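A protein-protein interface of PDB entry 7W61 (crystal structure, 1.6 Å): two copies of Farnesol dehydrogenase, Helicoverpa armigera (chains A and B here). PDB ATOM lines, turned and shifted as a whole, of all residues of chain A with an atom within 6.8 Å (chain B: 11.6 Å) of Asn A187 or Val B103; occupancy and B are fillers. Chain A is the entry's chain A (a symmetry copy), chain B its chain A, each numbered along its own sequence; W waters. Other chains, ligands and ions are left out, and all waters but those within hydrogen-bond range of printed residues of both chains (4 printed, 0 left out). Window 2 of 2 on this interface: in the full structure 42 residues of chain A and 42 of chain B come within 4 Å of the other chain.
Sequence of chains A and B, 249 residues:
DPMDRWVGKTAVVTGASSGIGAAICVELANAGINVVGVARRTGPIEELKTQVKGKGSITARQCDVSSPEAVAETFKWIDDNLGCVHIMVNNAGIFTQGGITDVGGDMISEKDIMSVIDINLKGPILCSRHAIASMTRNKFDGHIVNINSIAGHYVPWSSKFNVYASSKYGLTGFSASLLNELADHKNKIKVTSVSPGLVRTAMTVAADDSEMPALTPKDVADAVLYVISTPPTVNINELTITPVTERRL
No position is printed for both chains.
Of the 12 pairs that touch across the chains among the printed residues, none has its exchanged pair printed and touching as well.
OD2 of Asp A184 is in hydrogen-bond range of OG of Ser B159 (2.6 Å).
The side-chain carboxylate (OE1) of Glu A181 lies within hydrogen-bond range of the side-chain hydroxyl (OG1) of Thr B101 (2.7 Å).
The backbone NH (N) of Ile B100 lies within hydrogen-bond range of the side-chain carboxylate (OE2) of Glu A181, 2.7 Å away.
NE2 of His A185 sits at hydrogen-bond distance from OG of Ser B159 (3.2 Å).
The backbone NH (N) of Ile B108 lies within hydrogen-bond range of the backbone carbonyl oxygen (O) of Gly B99, 2.9 Å away.
O of Leu A182 sits at hydrogen-bond distance from N of Asn A187, at 2.9 Å.
OG1 of Thr B101 sits at hydrogen-bond distance from N of Val B103.
N of Gly B99 lies within hydrogen-bond range of O of Asp B106 (2.9 Å).
The side-chain hydroxyl of Thr A136 is in hydrogen-bond range of the backbone carbonyl oxygen of Ile A132.
The backbone NH of Ile A189 sits at hydrogen-bond distance from the side-chain amide oxygen of Asn A187 (2.9 Å).
Along chain A the printed residues that touch a printed residue of chain B span positions 132 to 187.
Printed residues of chain B that touch a printed residue of chain A: Gly B99, Ile B100, Thr B101, Val B103, Gly B104 and Ser B159.
Hydrophobic or aromatic side chains of chain B within 4 Å of the printed part of chain A: Ile B100 and Val B103.
Along chain B the printed residues that touch a printed residue of chain A span positions 99 to 159.
Among the printed residues, no Asp or Glu carboxylate lies within 4 Å of a Lys or Arg side-chain nitrogen of the other chain.
Water W3 lies within hydrogen-bond range of the side-chain carboxylate of Glu A181, the backbone carbonyl oxygen of Ser B159 and the backbone NH of Asn B162.
Water W4 lies within hydrogen-bond range of the backbone carbonyl oxygen (O) of His A185 and the backbone carbonyl oxygen (O) of Val B103.
Water W1 lies within hydrogen-bond range of the backbone carbonyl oxygen of Ser B159 (2.7 Å), the side-chain carboxylate of Asp B106 (2.8 Å) and a ring nitrogen (NE2) of His A185 (2.9 Å).
Water W2 bridges the side-chain carboxylate of Asp A184 (2.8 Å) and the backbone NH of Ser B159 (3.0 Å).
Thr B101 touches Ile A132 (CG2 to CD1, 3.8 Å).
Val B103 touches Thr A136 (CG1 to CG2, 3.8 Å).
Glu A181 touches Gly B99.
Glu A181 touches Ser B159 (CA to CB, 3.9 Å).
CD2 of Leu A182 touches CG1 of Val B103, 3.99 Å away.
His A185 touches Val B103.
His A185 touches Gly B104 (CE1 to CA, 3.5 Å).
Val B103 touches Asn A187 (CG1 to ND2, 3.8 Å).
Asn A187 touches just one residue of chain B: Val B103.
Printed residues of chain A within 4 Å of Val B103: Thr A136, Leu A182, His A185 and Asn A187.
Of chain B, only Gly B99 (3.3 Å), Ile B100 (2.7 Å), Thr B101 (2.7 Å) and Ser B159 (3.9 Å) come within 4 Å of Glu A181.
Of the printed residues of chain B, His A185 touches Val B103 (3.7 Å), Gly B104 (3.5 Å) and Ser B159 (3.2 Å).
No residue of chain B comes within 4 Å of Ile A189.
Of the printed residues of chain A, Gly B99 touches Glu A181 (3.3 Å).
Printed residues of chain A within 4 Å of Ile B100: Glu A181.
Of the printed residues of chain B, Leu A182 touches Val B103.
Printed residues of chain A within 4 Å of Thr B101: Ile A132 and Glu A181.
Of the printed residues of chain B, Ile A132 touches Thr B101 (3.8 Å).
Leu A179 touches none of the printed residues of chain B.
Lys A190 touches none of the printed residues of chain B.
The nearest residue of chain B that does not touch Asn A187 is Thr B101 (7.2 Å).
The nearest printed residue of chain A that does not touch Val B103 is Glu A181 (4.3 Å).
The nearest printed residue of chain A that does not touch Gly B99 is His A185 (6.3 Å).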
ATOM      1  N   ILE A 132      13.795   7.147  -9.480  1.00  0.00           N
ATOM      2  CA  ILE A 132      14.042   5.707  -9.397  1.00  0.00           C
ATOM      3  C   ILE A 132      13.967   5.106 -10.818  1.00  0.00           C
ATOM      4  O   ILE A 132      14.786   4.197 -11.080  1.00  0.00           O
ATOM      5  CB  ILE A 132      13.154   5.041  -8.354  1.00  0.00           C
ATOM      6  CG1 ILE A 132      13.564   5.555  -6.975  1.00  0.00           C
ATOM      7  CG2 ILE A 132      13.181   3.506  -8.522  1.00  0.00           C
ATOM      8  CD1 ILE A 132      12.599   5.109  -5.852  1.00  0.00           C
ATOM      9  N   THR A 136      17.156   2.913 -12.079  1.00  0.00           N
ATOM     10  CA  THR A 136      17.040   1.519 -12.486  1.00  0.00           C
ATOM     11  C   THR A 136      17.326   1.375 -14.000  1.00  0.00           C
ATOM     12  O   THR A 136      17.976   0.406 -14.387  1.00  0.00           O
ATOM     13  CB  THR A 136      15.741   0.859 -12.004  1.00  0.00           C
ATOM     14  OG1 THR A 136      14.715   1.596 -12.632  1.00  0.00           O
ATOM     15  CG2 THR A 136      15.506   0.882 -10.507  1.00  0.00           C
ATOM     16  N   PHE A 140      21.803   1.712 -11.446  1.00  0.00           N
ATOM     17  CA  PHE A 140      22.550   2.389 -10.400  1.00  0.00           C
ATOM     18  C   PHE A 140      21.741   2.410  -9.096  1.00  0.00           C
ATOM     19  O   PHE A 140      20.540   2.717  -9.113  1.00  0.00           O
ATOM     20  CB  PHE A 140      22.744   3.855 -10.836  1.00  0.00           C
ATOM     21  CG  PHE A 140      23.583   4.606  -9.830  1.00  0.00           C
ATOM     22  CD1 PHE A 140      24.971   4.453  -9.849  1.00  0.00           C
ATOM     23  CD2 PHE A 140      23.025   5.442  -8.857  1.00  0.00           C
ATOM     24  CE1 PHE A 140      25.775   5.129  -8.949  1.00  0.00           C
ATOM     25  CE2 PHE A 140      23.846   6.089  -7.915  1.00  0.00           C
ATOM     26  CZ  PHE A 140      25.204   5.915  -7.940  1.00  0.00           C
ATOM     27  N   ASP A 141      22.374   2.040  -7.978  1.00  0.00           N
ATOM     28  CA  ASP A 141      21.688   2.102  -6.663  1.00  0.00           C
ATOM     29  C   ASP A 141      21.942   3.459  -6.017  1.00  0.00           C
ATOM     30  O   ASP A 141      22.955   3.649  -5.302  1.00  0.00           O
ATOM     31  CB  ASP A 141      22.189   0.970  -5.744  1.00  0.00           C
ATOM     32  CG  ASP A 141      21.857  -0.398  -6.294  1.00  0.00           C
ATOM     33  OD1 ASP A 141      20.762  -0.576  -6.845  1.00  0.00           O
ATOM     34  OD2 ASP A 141      22.737  -1.287  -6.157  1.00  0.00           O
ATOM     35  N   GLY A 142      21.008   4.429  -6.224  1.00  0.00           N
ATOM     36  CA  GLY A 142      21.210   5.787  -5.687  1.00  0.00           C
ATOM     37  C   GLY A 142      20.527   5.955  -4.344  1.00  0.00           C
ATOM     38  O   GLY A 142      20.316   4.954  -3.621  1.00  0.00           O
ATOM     39  N   LEU A 179      10.843   2.469   0.824  1.00  0.00           N
ATOM     40  CA  LEU A 179      11.952   1.595   1.162  1.00  0.00           C
ATOM     41  C   LEU A 179      11.529   0.124   1.304  1.00  0.00           C
ATOM     42  O   LEU A 179      12.264  -0.753   0.811  1.00  0.00           O
ATOM     43  CB  LEU A 179      12.624   2.079   2.457  1.00  0.00           C
ATOM     44  CG  LEU A 179      13.891   1.288   2.827  1.00  0.00           C
ATOM     45  CD1 LEU A 179      15.014   1.585   1.797  1.00  0.00           C
ATOM     46  CD2 LEU A 179      14.349   1.818   4.230  1.00  0.00           C
ATOM     47  N   GLU A 181       9.190  -1.380  -0.449  1.00  0.00           N
ATOM     48  CA  GLU A 181       8.938  -1.896  -1.776  1.00  0.00           C
ATOM     49  C   GLU A 181      10.277  -2.213  -2.421  1.00  0.00           C
ATOM     50  O   GLU A 181      10.437  -3.303  -2.993  1.00  0.00           O
ATOM     51  CB  GLU A 181       8.222  -0.769  -2.527  1.00  0.00           C
ATOM     52  CG  GLU A 181       8.059  -1.126  -4.028  1.00  0.00           C
ATOM     53  CD  GLU A 181       7.289  -0.014  -4.716  1.00  0.00           C
ATOM     54  OE1 GLU A 181       7.737   0.391  -5.828  1.00  0.00           O
ATOM     55  OE2 GLU A 181       6.223   0.429  -4.238  1.00  0.00           O
ATOM     56  N   LEU A 182      11.255  -1.293  -2.308  1.00  0.00           N
ATOM     57  CA  LEU A 182      12.584  -1.564  -2.883  1.00  0.00           C
ATOM     58  C   LEU A 182      13.203  -2.834  -2.256  1.00  0.00           C
ATOM     59  O   LEU A 182      13.595  -3.759  -2.971  1.00  0.00           O
ATOM     60  CB  LEU A 182      13.454  -0.315  -2.680  1.00  0.00           C
ATOM     61  CG  LEU A 182      12.891   0.957  -3.331  1.00  0.00           C
ATOM     62  CD1 LEU A 182      13.751   2.120  -2.833  1.00  0.00           C
ATOM     63  CD2 LEU A 182      13.081   0.913  -4.880  1.00  0.00           C
ATOM     64  N   ALA A 183      13.104  -2.903  -0.921  1.00  0.00           N
ATOM     65  CA  ALA A 183      13.687  -4.069  -0.230  1.00  0.00           C
ATOM     66  C   ALA A 183      13.002  -5.377  -0.598  1.00  0.00           C
ATOM     67  O   ALA A 183      13.666  -6.421  -0.754  1.00  0.00           O
ATOM     68  CB  ALA A 183      13.569  -3.798   1.284  1.00  0.00           C
ATOM     69  N   ASP A 184      11.672  -5.344  -0.706  1.00  0.00           N
ATOM     70  CA  ASP A 184      10.925  -6.553  -1.007  1.00  0.00           C
ATOM     71  C   ASP A 184      11.334  -7.104  -2.380  1.00  0.00           C
ATOM     72  O   ASP A 184      11.315  -8.356  -2.575  1.00  0.00           O
ATOM     73  CB  ASP A 184       9.448  -6.228  -1.042  1.00  0.00           C
ATOM     74  CG  ASP A 184       8.601  -7.491  -1.085  1.00  0.00           C
ATOM     75  OD1 ASP A 184       8.895  -8.446  -0.317  1.00  0.00           O
ATOM     76  OD2 ASP A 184       7.703  -7.533  -1.858  1.00  0.00           O
ATOM     77  N   HIS A 185      11.760  -6.217  -3.311  1.00  0.00           N
ATOM     78  CA  HIS A 185      12.196  -6.688  -4.635  1.00  0.00           C
ATOM     79  C   HIS A 185      13.728  -6.772  -4.699  1.00  0.00           C
ATOM     80  O   HIS A 185      14.283  -6.856  -5.805  1.00  0.00           O
ATOM     81  CB  HIS A 185      11.665  -5.684  -5.648  1.00  0.00           C
ATOM     82  CG  HIS A 185      10.164  -5.741  -5.647  1.00  0.00           C
ATOM     83  ND1 HIS A 185       9.508  -6.913  -5.951  1.00  0.00           N
ATOM     84  CD2 HIS A 185       9.223  -4.780  -5.448  1.00  0.00           C
ATOM     85  CE1 HIS A 185       8.185  -6.657  -5.861  1.00  0.00           C
ATOM     86  NE2 HIS A 185       7.987  -5.380  -5.524  1.00  0.00           N
ATOM     87  N   LYS A 186      14.413  -6.728  -3.532  1.00  0.00           N
ATOM     88  CA  LYS A 186      15.866  -6.893  -3.495  1.00  0.00           C
ATOM     89  C   LYS A 186      16.614  -5.785  -4.252  1.00  0.00           C
ATOM     90  O   LYS A 186      17.764  -5.967  -4.685  1.00  0.00           O
ATOM     91  CB  LYS A 186      16.295  -8.298  -3.989  1.00  0.00           C
ATOM     92  CG  LYS A 186      16.020  -9.334  -2.881  1.00  0.00           C
ATOM     93  CD  LYS A 186      17.129  -9.183  -1.814  1.00  0.00           C
ATOM     94  CE  LYS A 186      17.290 -10.316  -0.783  1.00  0.00           C
ATOM     95  NZ  LYS A 186      18.091  -9.991   0.463  1.00  0.00           N
ATOM     96  N   ASN A 187      16.015  -4.588  -4.291  1.00  0.00           N
ATOM     97  CA  ASN A 187      16.656  -3.453  -4.890  1.00  0.00           C
ATOM     98  C   ASN A 187      17.342  -2.665  -3.774  1.00  0.00           C
ATOM     99  O   ASN A 187      16.790  -2.512  -2.669  1.00  0.00           O
ATOM    100  CB  ASN A 187      15.597  -2.585  -5.609  1.00  0.00           C
ATOM    101  CG  ASN A 187      16.237  -1.340  -6.199  1.00  0.00           C
ATOM    102  OD1 ASN A 187      16.428  -0.377  -5.476  1.00  0.00           O
ATOM    103  ND2 ASN A 187      16.532  -1.321  -7.498  1.00  0.00           N
ATOM    104  N   LYS A 188      18.536  -2.172  -4.083  1.00  0.00           N
ATOM    105  CA  LYS A 188      19.474  -1.593  -3.136  1.00  0.00           C
ATOM    106  C   LYS A 188      19.492  -0.071  -3.133  1.00  0.00           C
ATOM    107  O   LYS A 188      20.379   0.514  -2.454  1.00  0.00           O
ATOM    108  CB  LYS A 188      20.890  -2.135  -3.333  1.00  0.00           C
ATOM    109  CG  LYS A 188      20.878  -3.654  -3.083  1.00  0.00           C
ATOM    110  CD  LYS A 188      22.200  -4.359  -3.274  1.00  0.00           C
ATOM    111  CE  LYS A 188      22.731  -4.198  -4.690  1.00  0.00           C
ATOM    112  NZ  LYS A 188      21.879  -4.830  -5.741  1.00  0.00           N
ATOM    113  N   ILE A 189      18.491   0.568  -3.735  1.00  0.00           N
ATOM    114  CA  ILE A 189      18.416   2.039  -3.594  1.00  0.00           C
ATOM    115  C   ILE A 189      18.066   2.380  -2.141  1.00  0.00           C
ATOM    116  O   ILE A 189      17.204   1.699  -1.509  1.00  0.00           O
ATOM    117  CB  ILE A 189      17.307   2.516  -4.540  1.00  0.00           C
ATOM    118  CG1 ILE A 189      17.816   2.403  -5.975  1.00  0.00           C
ATOM    119  CG2 ILE A 189      16.909   3.975  -4.222  1.00  0.00           C
ATOM    120  CD1 ILE A 189      16.712   2.557  -7.076  1.00  0.00           C
ATOM    121  N   LYS A 190      18.716   3.424  -1.642  1.00  0.00           N
ATOM    122  CA  LYS A 190      18.519   3.847  -0.239  1.00  0.00           C
ATOM    123  C   LYS A 190      17.457   4.943  -0.146  1.00  0.00           C
ATOM    124  O   LYS A 190      17.309   5.723  -1.078  1.00  0.00           O
ATOM    125  CB  LYS A 190      19.867   4.394   0.293  1.00  0.00           C
ATOM    126  CG  LYS A 190      20.854   3.217   0.440  1.00  0.00           C
ATOM    127  CD  LYS A 190      22.321   3.476   0.852  1.00  0.00           C
ATOM    128  CE  LYS A 190      22.467   4.372   2.030  1.00  0.00           C
ATOM    129  NZ  LYS A 190      23.913   4.498   2.401  1.00  0.00           N
ATOM    130  N   GLY B  98      -0.223  -2.652  -6.248  1.00  0.00           N
ATOM    131  CA  GLY B  98       1.034  -2.621  -6.968  1.00  0.00           C
ATOM    132  C   GLY B  98       2.017  -1.605  -6.415  1.00  0.00           C
ATOM    133  O   GLY B  98       1.869  -1.207  -5.273  1.00  0.00           O
ATOM    134  N   GLY B  99       3.010  -1.215  -7.227  1.00  0.00           N
ATOM    135  CA  GLY B  99       4.153  -0.497  -6.637  1.00  0.00           C
ATOM    136  C   GLY B  99       4.145   0.994  -6.954  1.00  0.00           C
ATOM    137  O   GLY B  99       3.510   1.436  -7.919  1.00  0.00           O
ATOM    138  N   ILE B 100       4.889   1.749  -6.130  1.00  0.00           N
ATOM    139  CA  ILE B 100       5.177   3.148  -6.457  1.00  0.00           C
ATOM    140  C   ILE B 100       6.027   3.177  -7.725  1.00  0.00           C
ATOM    141  O   ILE B 100       5.884   4.077  -8.546  1.00  0.00           O
ATOM    142  CB  ILE B 100       5.946   3.739  -5.256  1.00  0.00           C
ATOM    143  CG1 ILE B 100       5.057   3.794  -4.007  1.00  0.00           C
ATOM    144  CG2 ILE B 100       6.499   5.136  -5.601  1.00  0.00           C
ATOM    145  CD1 ILE B 100       5.812   3.733  -2.653  1.00  0.00           C
ATOM    146  N   THR B 101       7.019   2.270  -7.779  1.00  0.00           N
ATOM    147  CA  THR B 101       7.998   2.199  -8.874  1.00  0.00           C
ATOM    148  C   THR B 101       7.770   0.881  -9.614  1.00  0.00           C
ATOM    149  O   THR B 101       6.898   0.093  -9.252  1.00  0.00           O
ATOM    150  CB  THR B 101       9.415   2.184  -8.312  1.00  0.00           C
ATOM    151  OG1 THR B 101       9.612   0.890  -7.761  1.00  0.00           O
ATOM    152  CG2 THR B 101       9.615   3.247  -7.236  1.00  0.00           C
ATOM    153  N   ASP B 102       8.622   0.624 -10.634  1.00  0.00           N
ATOM    154  CA  ASP B 102       8.492  -0.595 -11.403  1.00  0.00           C
ATOM    155  C   ASP B 102       9.531  -1.637 -11.038  1.00  0.00           C
ATOM    156  O   ASP B 102       9.786  -2.582 -11.857  1.00  0.00           O
ATOM    157  CB  ASP B 102       8.472  -0.283 -12.927  1.00  0.00           C
ATOM    158  CG  ASP B 102       7.699  -1.346 -13.691  1.00  0.00           C
ATOM    159  OD1 ASP B 102       8.012  -1.503 -14.943  1.00  0.00           O
ATOM    160  OD2 ASP B 102       6.719  -1.956 -13.182  1.00  0.00           O
ATOM    161  N   VAL B 103      10.147  -1.508  -9.825  1.00  0.00           N
ATOM    162  CA  VAL B 103      11.242  -2.438  -9.499  1.00  0.00           C
ATOM    163  C   VAL B 103      10.746  -3.883  -9.411  1.00  0.00           C
ATOM    164  O   VAL B 103      11.564  -4.819  -9.570  1.00  0.00           O
ATOM    165  CB  VAL B 103      12.037  -2.126  -8.236  1.00  0.00           C
ATOM    166  CG1 VAL B 103      12.835  -0.869  -8.440  1.00  0.00           C
ATOM    167  CG2 VAL B 103      11.099  -1.997  -7.052  1.00  0.00           C
ATOM    168  N   GLY B 104       9.453  -4.103  -9.207  1.00  0.00           N
ATOM    169  CA  GLY B 104       8.847  -5.424  -9.096  1.00  0.00           C
ATOM    170  C   GLY B 104       7.968  -5.719 -10.304  1.00  0.00           C
ATOM    171  O   GLY B 104       7.275  -6.752 -10.319  1.00  0.00           O
ATOM    172  N   GLY B 105       8.030  -4.827 -11.298  1.00  0.00           N
ATOM    173  CA  GLY B 105       7.203  -5.085 -12.481  1.00  0.00           C
ATOM    174  C   GLY B 105       5.697  -4.916 -12.264  1.00  0.00           C
ATOM    175  O   GLY B 105       4.879  -5.409 -13.045  1.00  0.00           O
ATOM    176  N   ASP B 106       5.318  -4.136 -11.225  1.00  0.00           N
ATOM    177  CA  ASP B 106       3.900  -3.933 -10.937  1.00  0.00           C
ATOM    178  C   ASP B 106       3.636  -2.477 -10.587  1.00  0.00           C
ATOM    179  O   ASP B 106       2.671  -2.191  -9.898  1.00  0.00           O
ATOM    180  CB  ASP B 106       3.377  -4.834  -9.797  1.00  0.00           C
ATOM    181  CG  ASP B 106       4.008  -4.617  -8.409  1.00  0.00           C
ATOM    182  OD1 ASP B 106       4.872  -3.750  -8.262  1.00  0.00           O
ATOM    183  OD2 ASP B 106       3.626  -5.384  -7.496  1.00  0.00           O
ATOM    184  N   MET B 107       4.340  -1.560 -11.236  1.00  0.00           N
ATOM    185  CA  MET B 107       4.136  -0.110 -10.964  1.00  0.00           C
ATOM    186  C   MET B 107       2.676   0.264 -11.294  1.00  0.00           C
ATOM    187  O   MET B 107       2.174  -0.072 -12.381  1.00  0.00           O
ATOM    188  CB  MET B 107       5.129   0.706 -11.856  1.00  0.00           C
ATOM    189  CG  MET B 107       4.970   2.222 -11.537  1.00  0.00           C
ATOM    190  SD  MET B 107       6.281   3.130 -12.434  1.00  0.00           S
ATOM    191  CE  MET B 107       6.623   4.608 -11.514  1.00  0.00           C
ATOM    192  N   ILE B 108       1.994   0.999 -10.401  1.00  0.00           N
ATOM    193  CA  ILE B 108       0.680   1.568 -10.720  1.00  0.00           C
ATOM    194  C   ILE B 108       0.821   2.859 -11.519  1.00  0.00           C
ATOM    195  O   ILE B 108       1.880   3.511 -11.503  1.00  0.00           O
ATOM    196  CB  ILE B 108      -0.227   1.737  -9.471  1.00  0.00           C
ATOM    197  CG1 ILE B 108       0.288   2.853  -8.537  1.00  0.00           C
ATOM    198  CG2 ILE B 108      -0.238   0.399  -8.751  1.00  0.00           C
ATOM    199  CD1 ILE B 108      -0.764   3.138  -7.445  1.00  0.00           C
ATOM    200  N   ILE B 113      -1.845   6.612  -8.772  1.00  0.00           N
ATOM    201  CA  ILE B 113      -1.076   6.963  -7.558  1.00  0.00           C
ATOM    202  C   ILE B 113      -1.483   8.356  -7.073  1.00  0.00           C
ATOM    203  O   ILE B 113      -1.624   8.610  -5.836  1.00  0.00           O
ATOM    204  CB  ILE B 113       0.460   6.754  -7.775  1.00  0.00           C
ATOM    205  CG1 ILE B 113       1.144   6.571  -6.406  1.00  0.00           C
ATOM    206  CG2 ILE B 113       1.095   7.909  -8.547  1.00  0.00           C
ATOM    207  CD1 ILE B 113       2.561   5.927  -6.560  1.00  0.00           C
ATOM    208  N   TRP B 157       3.954  -4.795   5.158  1.00  0.00           N
ATOM    209  CA  TRP B 157       5.084  -5.545   4.614  1.00  0.00           C
ATOM    210  C   TRP B 157       4.867  -5.746   3.129  1.00  0.00           C
ATOM    211  O   TRP B 157       5.808  -5.734   2.337  1.00  0.00           O
ATOM    212  CB  TRP B 157       5.155  -6.955   5.213  1.00  0.00           C
ATOM    213  CG  TRP B 157       5.928  -6.990   6.494  1.00  0.00           C
ATOM    214  CD1 TRP B 157       7.229  -7.376   6.606  1.00  0.00           C
ATOM    215  CD2 TRP B 157       5.496  -6.668   7.831  1.00  0.00           C
ATOM    216  NE1 TRP B 157       7.633  -7.345   7.907  1.00  0.00           N
ATOM    217  CE2 TRP B 157       6.581  -6.947   8.697  1.00  0.00           C
ATOM    218  CE3 TRP B 157       4.283  -6.251   8.384  1.00  0.00           C
ATOM    219  CZ2 TRP B 157       6.543  -6.665  10.063  1.00  0.00           C
ATOM    220  CZ3 TRP B 157       4.240  -5.961   9.743  1.00  0.00           C
ATOM    221  CH2 TRP B 157       5.343  -6.189  10.567  1.00  0.00           C
ATOM    222  N   SER B 158       3.593  -5.942   2.794  1.00  0.00           N
ATOM    223  CA  SER B 158       3.304  -6.178   1.376  1.00  0.00           C
ATOM    224  C   SER B 158       3.767  -5.020   0.504  1.00  0.00           C
ATOM    225  O   SER B 158       3.356  -3.877   0.747  1.00  0.00           O
ATOM    226  CB  SER B 158       1.880  -6.483   1.160  1.00  0.00           C
ATOM    227  OG  SER B 158       1.560  -6.444  -0.263  1.00  0.00           O
ATOM    228  N   SER B 159       4.464  -5.340  -0.601  1.00  0.00           N
ATOM    229  CA  SER B 159       4.838  -4.281  -1.529  1.00  0.00           C
ATOM    230  C   SER B 159       3.719  -3.998  -2.532  1.00  0.00           C
ATOM    231  O   SER B 159       3.979  -3.284  -3.520  1.00  0.00           O
ATOM    232  CB  SER B 159       6.142  -4.589  -2.185  1.00  0.00           C
ATOM    233  OG  SER B 159       6.050  -5.806  -2.979  1.00  0.00           O
ATOM    234  N   LYS B 160       2.498  -4.491  -2.271  1.00  0.00           N
ATOM    235  CA  LYS B 160       1.400  -4.076  -3.158  1.00  0.00           C
ATOM    236  C   LYS B 160       0.748  -2.780  -2.663  1.00  0.00           C
ATOM    237  O   LYS B 160      -0.203  -2.270  -3.271  1.00  0.00           O
ATOM    238  CB  LYS B 160       0.309  -5.161  -3.151  1.00  0.00           C
ATOM    239  CG  LYS B 160       0.799  -6.473  -3.858  1.00  0.00           C
ATOM    240  CD  LYS B 160       0.949  -6.243  -5.390  1.00  0.00           C
ATOM    241  CE  LYS B 160       1.439  -7.520  -6.079  1.00  0.00           C
ATOM    242  NZ  LYS B 160       1.625  -7.300  -7.525  1.00  0.00           N
ATOM    243  N   PHE B 161       1.242  -2.256  -1.542  1.00  0.00           N
ATOM    244  CA  PHE B 161       0.500  -1.151  -0.922  1.00  0.00           C
ATOM    245  C   PHE B 161       0.886   0.251  -1.376  1.00  0.00           C
ATOM    246  O   PHE B 161       0.070   1.162  -1.073  1.00  0.00           O
ATOM    247  CB  PHE B 161       0.619  -1.175   0.616  1.00  0.00           C
ATOM    248  CG  PHE B 161      -0.443  -2.124   1.169  1.00  0.00           C
ATOM    249  CD1 PHE B 161      -0.293  -3.513   1.143  1.00  0.00           C
ATOM    250  CD2 PHE B 161      -1.590  -1.588   1.708  1.00  0.00           C
ATOM    251  CE1 PHE B 161      -1.260  -4.378   1.593  1.00  0.00           C
ATOM    252  CE2 PHE B 161      -2.571  -2.474   2.167  1.00  0.00           C
ATOM    253  CZ  PHE B 161      -2.421  -3.850   2.103  1.00  0.00           C
ATOM    254  N   ASN B 162       1.997   0.463  -2.124  1.00  0.00           N
ATOM    255  CA  ASN B 162       2.305   1.769  -2.739  1.00  0.00           C
ATOM    256  C   ASN B 162       2.084   2.912  -1.732  1.00  0.00           C
ATOM    257  O   ASN B 162       2.791   2.960  -0.706  1.00  0.00           O
ATOM    258  CB  ASN B 162       1.675   1.999  -4.140  1.00  0.00           C
ATOM    259  CG  ASN B 162       0.175   1.811  -4.182  1.00  0.00           C
ATOM    260  OD1 ASN B 162      -0.554   2.767  -3.920  1.00  0.00           O
ATOM    261  ND2 ASN B 162      -0.306   0.603  -4.480  1.00  0.00           N
HETATM  262  O   HOH W   1       5.725  -3.641  -5.599  1.00  0.00           O
HETATM  263  O   HOH W   2       5.194  -8.220  -0.851  1.00  0.00           O
HETATM  264  O   HOH W   3       4.611  -0.776  -2.510  1.00  0.00           O
HETATM  265  O   HOH W   4      14.296  -5.352  -7.995  1.00  0.00           O
